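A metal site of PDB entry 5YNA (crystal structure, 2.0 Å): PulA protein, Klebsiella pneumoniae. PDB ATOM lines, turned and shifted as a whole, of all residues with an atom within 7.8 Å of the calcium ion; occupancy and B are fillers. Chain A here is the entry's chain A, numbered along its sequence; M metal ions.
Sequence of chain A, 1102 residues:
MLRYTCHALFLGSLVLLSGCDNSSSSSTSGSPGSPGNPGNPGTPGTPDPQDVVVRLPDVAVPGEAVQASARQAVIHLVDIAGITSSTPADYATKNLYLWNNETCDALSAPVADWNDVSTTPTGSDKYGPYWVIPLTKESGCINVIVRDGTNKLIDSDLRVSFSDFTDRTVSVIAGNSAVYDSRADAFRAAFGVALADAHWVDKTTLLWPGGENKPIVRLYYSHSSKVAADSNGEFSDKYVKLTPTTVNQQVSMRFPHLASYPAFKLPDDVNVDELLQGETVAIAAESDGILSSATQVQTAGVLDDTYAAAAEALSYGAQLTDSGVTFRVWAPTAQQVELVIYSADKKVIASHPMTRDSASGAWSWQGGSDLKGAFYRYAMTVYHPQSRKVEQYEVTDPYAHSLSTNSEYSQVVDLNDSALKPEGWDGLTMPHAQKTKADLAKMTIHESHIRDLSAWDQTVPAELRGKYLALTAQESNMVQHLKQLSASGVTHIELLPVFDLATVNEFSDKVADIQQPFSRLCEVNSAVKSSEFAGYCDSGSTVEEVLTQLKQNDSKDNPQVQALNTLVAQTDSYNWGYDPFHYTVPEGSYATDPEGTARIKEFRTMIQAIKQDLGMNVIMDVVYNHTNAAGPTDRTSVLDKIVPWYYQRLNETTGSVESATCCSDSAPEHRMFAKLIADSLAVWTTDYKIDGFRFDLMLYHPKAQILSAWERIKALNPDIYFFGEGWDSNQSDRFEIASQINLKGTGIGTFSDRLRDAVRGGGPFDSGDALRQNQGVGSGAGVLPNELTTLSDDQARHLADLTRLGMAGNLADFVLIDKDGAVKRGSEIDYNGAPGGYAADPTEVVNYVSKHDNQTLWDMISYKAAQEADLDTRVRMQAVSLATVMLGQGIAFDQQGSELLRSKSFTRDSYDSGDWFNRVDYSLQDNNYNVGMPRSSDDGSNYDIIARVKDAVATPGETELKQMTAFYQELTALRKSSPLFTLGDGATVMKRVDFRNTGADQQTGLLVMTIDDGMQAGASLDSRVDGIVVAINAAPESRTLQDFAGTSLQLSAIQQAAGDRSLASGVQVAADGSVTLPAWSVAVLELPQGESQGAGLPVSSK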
ATOM      1  N   LEU A 980       9.914  10.597  28.126  1.00  0.00           N
ATOM      2  CA  LEU A 980       8.977  11.642  27.716  1.00  0.00           C
ATOM      3  C   LEU A 980       7.690  11.589  28.518  1.00  0.00           C
ATOM      4  O   LEU A 980       7.020  12.618  28.697  1.00  0.00           O
ATOM      5  CB  LEU A 980       8.678  11.507  26.222  1.00  0.00           C
ATOM      6  CG  LEU A 980       9.884  11.805  25.320  1.00  0.00           C
ATOM      7  CD1 LEU A 980       9.561  11.502  23.874  1.00  0.00           C
ATOM      8  CD2 LEU A 980      10.306  13.262  25.523  1.00  0.00           C
ATOM      9  N   ARG A 992       7.014  20.861  25.862  1.00  0.00           N
ATOM     10  CA  ARG A 992       7.051  19.637  25.055  1.00  0.00           C
ATOM     11  C   ARG A 992       5.698  18.954  24.834  1.00  0.00           C
ATOM     12  O   ARG A 992       5.590  18.147  23.909  1.00  0.00           O
ATOM     13  CB  ARG A 992       8.026  18.627  25.673  1.00  0.00           C
ATOM     14  CG  ARG A 992       9.457  19.154  25.700  1.00  0.00           C
ATOM     15  CD  ARG A 992      10.379  18.371  26.649  1.00  0.00           C
ATOM     16  NE  ARG A 992      11.303  17.496  25.921  1.00  0.00           N
ATOM     17  CZ  ARG A 992      12.592  17.737  25.721  1.00  0.00           C
ATOM     18  NH1 ARG A 992      13.314  16.850  25.054  1.00  0.00           N
ATOM     19  NH2 ARG A 992      13.171  18.846  26.199  1.00  0.00           N
ATOM     20  N   ASP A1012       6.907  16.330  22.599  1.00  0.00           N
ATOM     21  CA  ASP A1012       7.982  16.677  21.675  1.00  0.00           C
ATOM     22  C   ASP A1012       9.330  16.176  22.178  1.00  0.00           C
ATOM     23  O   ASP A1012       9.663  16.301  23.362  1.00  0.00           O
ATOM     24  CB  ASP A1012       8.023  18.202  21.538  1.00  0.00           C
ATOM     25  CG  ASP A1012       8.899  18.659  20.401  1.00  0.00           C
ATOM     26  OD1 ASP A1012       9.394  17.812  19.624  1.00  0.00           O
ATOM     27  OD2 ASP A1012       9.100  19.893  20.315  1.00  0.00           O
ATOM     28  N   ASP A1013      10.106  15.568  21.279  1.00  0.00           N
ATOM     29  CA  ASP A1013      11.527  15.358  21.539  1.00  0.00           C
ATOM     30  C   ASP A1013      12.384  15.778  20.343  1.00  0.00           C
ATOM     31  O   ASP A1013      13.376  15.123  20.005  1.00  0.00           O
ATOM     32  CB  ASP A1013      11.830  13.905  21.881  1.00  0.00           C
ATOM     33  CG  ASP A1013      12.949  13.794  22.889  1.00  0.00           C
ATOM     34  OD1 ASP A1013      13.088  14.696  23.749  1.00  0.00           O
ATOM     35  OD2 ASP A1013      13.697  12.806  22.797  1.00  0.00           O
ATOM     36  N   GLY A1014      11.994  16.876  19.697  1.00  0.00           N
ATOM     37  CA  GLY A1014      12.759  17.465  18.615  1.00  0.00           C
ATOM     38  C   GLY A1014      13.369  18.794  19.012  1.00  0.00           C
ATOM     39  O   GLY A1014      13.281  19.251  20.164  1.00  0.00           O
ATOM     40  N   GLY A1018      14.377  21.476  22.911  1.00  0.00           N
ATOM     41  CA  GLY A1018      15.654  21.433  23.595  1.00  0.00           C
ATOM     42  C   GLY A1018      16.371  20.134  23.307  1.00  0.00           C
ATOM     43  O   GLY A1018      16.401  19.674  22.166  1.00  0.00           O
ATOM     44  N   ALA A1019      16.943  19.525  24.341  1.00  0.00           N
ATOM     45  CA  ALA A1019      17.708  18.297  24.189  1.00  0.00           C
ATOM     46  C   ALA A1019      16.787  17.110  23.898  1.00  0.00           C
ATOM     47  O   ALA A1019      15.607  17.092  24.257  1.00  0.00           O
ATOM     48  CB  ALA A1019      18.510  18.030  25.467  1.00  0.00           C
ATOM     49  N   SER A1020      17.361  16.079  23.278  1.00  0.00           N
ATOM     50  CA  SER A1020      16.626  14.838  23.028  1.00  0.00           C
ATOM     51  C   SER A1020      16.700  13.954  24.267  1.00  0.00           C
ATOM     52  O   SER A1020      17.674  13.220  24.453  1.00  0.00           O
ATOM     53  CB  SER A1020      17.181  14.109  21.815  1.00  0.00           C
ATOM     54  OG  SER A1020      16.983  12.715  21.927  1.00  0.00           O
ATOM     55  N   LEU A1021      15.663  14.005  25.103  1.00  0.00           N
ATOM     56  CA  LEU A1021      15.606  13.192  26.320  1.00  0.00           C
ATOM     57  C   LEU A1021      15.474  11.697  26.027  1.00  0.00           C
ATOM     58  O   LEU A1021      15.666  10.891  26.932  1.00  0.00           O
ATOM     59  CB  LEU A1021      14.429  13.631  27.190  1.00  0.00           C
ATOM     60  CG  LEU A1021      14.422  15.123  27.505  1.00  0.00           C
ATOM     61  CD1 LEU A1021      13.180  15.526  28.317  1.00  0.00           C
ATOM     62  CD2 LEU A1021      15.704  15.526  28.229  1.00  0.00           C
ATOM     63  N   ASP A1022      15.139  11.319  24.794  1.00  0.00           N
ATOM     64  CA  ASP A1022      14.979   9.916  24.427  1.00  0.00           C
ATOM     65  C   ASP A1022      15.756   9.690  23.150  1.00  0.00           C
ATOM     66  O   ASP A1022      15.471  10.323  22.123  1.00  0.00           O
ATOM     67  CB  ASP A1022      13.501   9.566  24.222  1.00  0.00           C
ATOM     68  CG  ASP A1022      13.266   8.076  24.049  1.00  0.00           C
ATOM     69  OD1 ASP A1022      14.162   7.364  23.544  1.00  0.00           O
ATOM     70  OD2 ASP A1022      12.157   7.608  24.428  1.00  0.00           O
ATOM     71  N   SER A1023      16.740   8.784  23.193  1.00  0.00           N
ATOM     72  CA  SER A1023      17.542   8.503  22.009  1.00  0.00           C
ATOM     73  C   SER A1023      16.747   7.770  20.925  1.00  0.00           C
ATOM     74  O   SER A1023      17.158   7.796  19.760  1.00  0.00           O
ATOM     75  CB  SER A1023      18.779   7.692  22.386  1.00  0.00           C
ATOM     76  OG  SER A1023      18.452   6.316  22.599  1.00  0.00           O
ATOM     77  N   ARG A1024      15.636   7.130  21.282  1.00  0.00           N
ATOM     78  CA  ARG A1024      14.943   6.256  20.354  1.00  0.00           C
ATOM     79  C   ARG A1024      13.843   6.950  19.560  1.00  0.00           C
ATOM     80  O   ARG A1024      13.436   6.427  18.525  1.00  0.00           O
ATOM     81  CB  ARG A1024      14.331   5.063  21.091  1.00  0.00           C
ATOM     82  CG  ARG A1024      15.116   3.766  20.933  1.00  0.00           C
ATOM     83  CD  ARG A1024      14.564   2.709  21.864  1.00  0.00           C
ATOM     84  NE  ARG A1024      14.186   3.287  23.142  1.00  0.00           N
ATOM     85  CZ  ARG A1024      13.820   2.592  24.217  1.00  0.00           C
ATOM     86  NH1 ARG A1024      13.492   3.214  25.343  1.00  0.00           N
ATOM     87  NH2 ARG A1024      13.776   1.265  24.165  1.00  0.00           N
ATOM     88  N   VAL A1025      13.349   8.101  20.023  1.00  0.00           N
ATOM     89  CA  VAL A1025      12.198   8.727  19.393  1.00  0.00           C
ATOM     90  C   VAL A1025      12.383  10.246  19.355  1.00  0.00           C
ATOM     91  O   VAL A1025      12.980  10.840  20.256  1.00  0.00           O
ATOM     92  CB  VAL A1025      10.867   8.363  20.109  1.00  0.00           C
ATOM     93  CG1 VAL A1025      10.673   6.852  20.197  1.00  0.00           C
ATOM     94  CG2 VAL A1025      10.810   9.009  21.493  1.00  0.00           C
ATOM     95  N   ASP A1026      11.856  10.851  18.291  1.00  0.00           N
ATOM     96  CA  ASP A1026      11.765  12.302  18.188  1.00  0.00           C
ATOM     97  C   ASP A1026      10.442  12.839  18.724  1.00  0.00           C
ATOM     98  O   ASP A1026      10.303  14.065  18.861  1.00  0.00           O
ATOM     99  CB  ASP A1026      11.932  12.746  16.736  1.00  0.00           C
ATOM    100  CG  ASP A1026      13.389  12.767  16.274  1.00  0.00           C
ATOM    101  OD1 ASP A1026      14.253  13.242  17.048  1.00  0.00           O
ATOM    102  OD2 ASP A1026      13.660  12.290  15.152  1.00  0.00           O
ATOM    103  N   GLY A1027       9.500  11.968  19.049  1.00  0.00           N
ATOM    104  CA  GLY A1027       8.217  12.391  19.570  1.00  0.00           C
ATOM    105  C   GLY A1027       7.343  11.185  19.889  1.00  0.00           C
ATOM    106  O   GLY A1027       7.583  10.070  19.416  1.00  0.00           O
ATOM    107  N   LEU A1087       7.683   8.650  16.675  1.00  0.00           N
ATOM    108  CA  LEU A1087       8.523   8.979  15.534  1.00  0.00           C
ATOM    109  C   LEU A1087       9.917   8.452  15.808  1.00  0.00           C
ATOM    110  O   LEU A1087      10.605   8.984  16.700  1.00  0.00           O
ATOM    111  CB  LEU A1087       8.554  10.482  15.317  1.00  0.00           C
ATOM    112  CG  LEU A1087       7.183  11.121  15.269  1.00  0.00           C
ATOM    113  CD1 LEU A1087       7.280  12.667  15.270  1.00  0.00           C
ATOM    114  CD2 LEU A1087       6.493  10.594  13.995  1.00  0.00           C
ATOM    115  N   PRO A1088      10.392   7.425  15.079  1.00  0.00           N
ATOM    116  CA  PRO A1088      11.742   6.899  15.333  1.00  0.00           C
ATOM    117  C   PRO A1088      12.803   7.949  15.089  1.00  0.00           C
ATOM    118  O   PRO A1088      12.717   8.739  14.144  1.00  0.00           O
ATOM    119  CB  PRO A1088      11.866   5.743  14.332  1.00  0.00           C
ATOM    120  CG  PRO A1088      10.485   5.379  13.977  1.00  0.00           C
ATOM    121  CD  PRO A1088       9.676   6.651  14.057  1.00  0.00           C
ATOM    122  N   GLN A1089      13.810   7.961  15.952  1.00  0.00           N
ATOM    123  CA  GLN A1089      14.887   8.938  15.822  1.00  0.00           C
ATOM    124  C   GLN A1089      15.876   8.502  14.743  1.00  0.00           C
ATOM    125  O   GLN A1089      16.091   7.310  14.504  1.00  0.00           O
ATOM    126  CB  GLN A1089      15.605   9.144  17.149  1.00  0.00           C
ATOM    127  CG  GLN A1089      16.206  10.531  17.244  1.00  0.00           C
ATOM    128  CD  GLN A1089      16.476  10.941  18.656  1.00  0.00           C
ATOM    129  OE1 GLN A1089      15.586  10.844  19.507  1.00  0.00           O
ATOM    130  NE2 GLN A1089      17.678  11.434  18.926  1.00  0.00           N
ATOM    131  N   GLY A1090      16.444   9.494  14.065  1.00  0.00           N
ATOM    132  CA  GLY A1090      17.483   9.298  13.085  1.00  0.00           C
ATOM    133  C   GLY A1090      18.863   9.502  13.668  1.00  0.00           C
ATOM    134  O   GLY A1090      19.081   9.417  14.881  1.00  0.00           O
ATOM    135  N   SER A1092      20.469  12.124  14.102  1.00  0.00           N
ATOM    136  CA  SER A1092      20.449  13.177  15.106  1.00  0.00           C
ATOM    137  C   SER A1092      19.003  13.588  15.409  1.00  0.00           C
ATOM    138  O   SER A1092      18.061  13.182  14.722  1.00  0.00           O
ATOM    139  CB  SER A1092      21.291  14.384  14.677  1.00  0.00           C
ATOM    140  OG  SER A1092      21.181  14.618  13.286  1.00  0.00           O
ATOM    141  N   GLN A1093      18.857  14.393  16.465  1.00  0.00           N
ATOM    142  CA  GLN A1093      17.568  14.907  16.922  1.00  0.00           C
ATOM    143  C   GLN A1093      16.786  15.546  15.778  1.00  0.00           C
ATOM    144  O   GLN A1093      17.196  16.586  15.239  1.00  0.00           O
ATOM    145  CB  GLN A1093      17.797  15.899  18.078  1.00  0.00           C
ATOM    146  CG  GLN A1093      16.616  16.773  18.458  1.00  0.00           C
ATOM    147  CD  GLN A1093      16.946  17.721  19.615  1.00  0.00           C
ATOM    148  OE1 GLN A1093      17.864  18.536  19.523  1.00  0.00           O
ATOM    149  NE2 GLN A1093      16.190  17.606  20.707  1.00  0.00           N
ATOM    150  N   GLY A1094      15.672  14.918  15.383  1.00  0.00           N
ATOM    151  CA  GLY A1094      14.839  15.405  14.297  1.00  0.00           C
ATOM    152  C   GLY A1094      13.952  16.564  14.712  1.00  0.00           C
ATOM    153  O   GLY A1094      14.116  17.187  15.765  1.00  0.00           O
HETATM  154 CA    CA M   1      14.846  12.203  21.024  1.00  0.00          CA
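The side-chain amide oxygen (OE1) of Gln 1089 lies close to the backbone carbonyl oxygen (O) of Ser 1023.
N of Gln 1089 sits at hydrogen-bond distance from O of Arg 1024, at 3.0 Å.
O of Asp 1026 sits at hydrogen-bond distance from N of Asp 1013.
The side-chain carboxylate (OD1) of Asp 1013 is in hydrogen-bond range of the backbone NH (N) of Leu 1021, at 3.0 Å.
OD1 of Asp 1013 lies within salt-bridge range of NH1 of Arg 992.
The side-chain carboxylate (OD1) of Asp 1022 lies within hydrogen-bond range of the backbone NH (N) of Arg 1024, at 2.7 Å.
N of Ser 1020 sits close to NE2 of Gln 1093, at 3.2 Å.
Of the 22 residues printed, 5 come within 4 Å of the calcium ion.
The calcium ion is bound by OE1 of Gln 1089 (2.2 Å), OD2 of Asp 1013 (2.2 Å), O of Asp 1022 (2.3 Å), OG of Ser 1020 (2.4 Å) and O of Val 1025 (2.4 Å).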
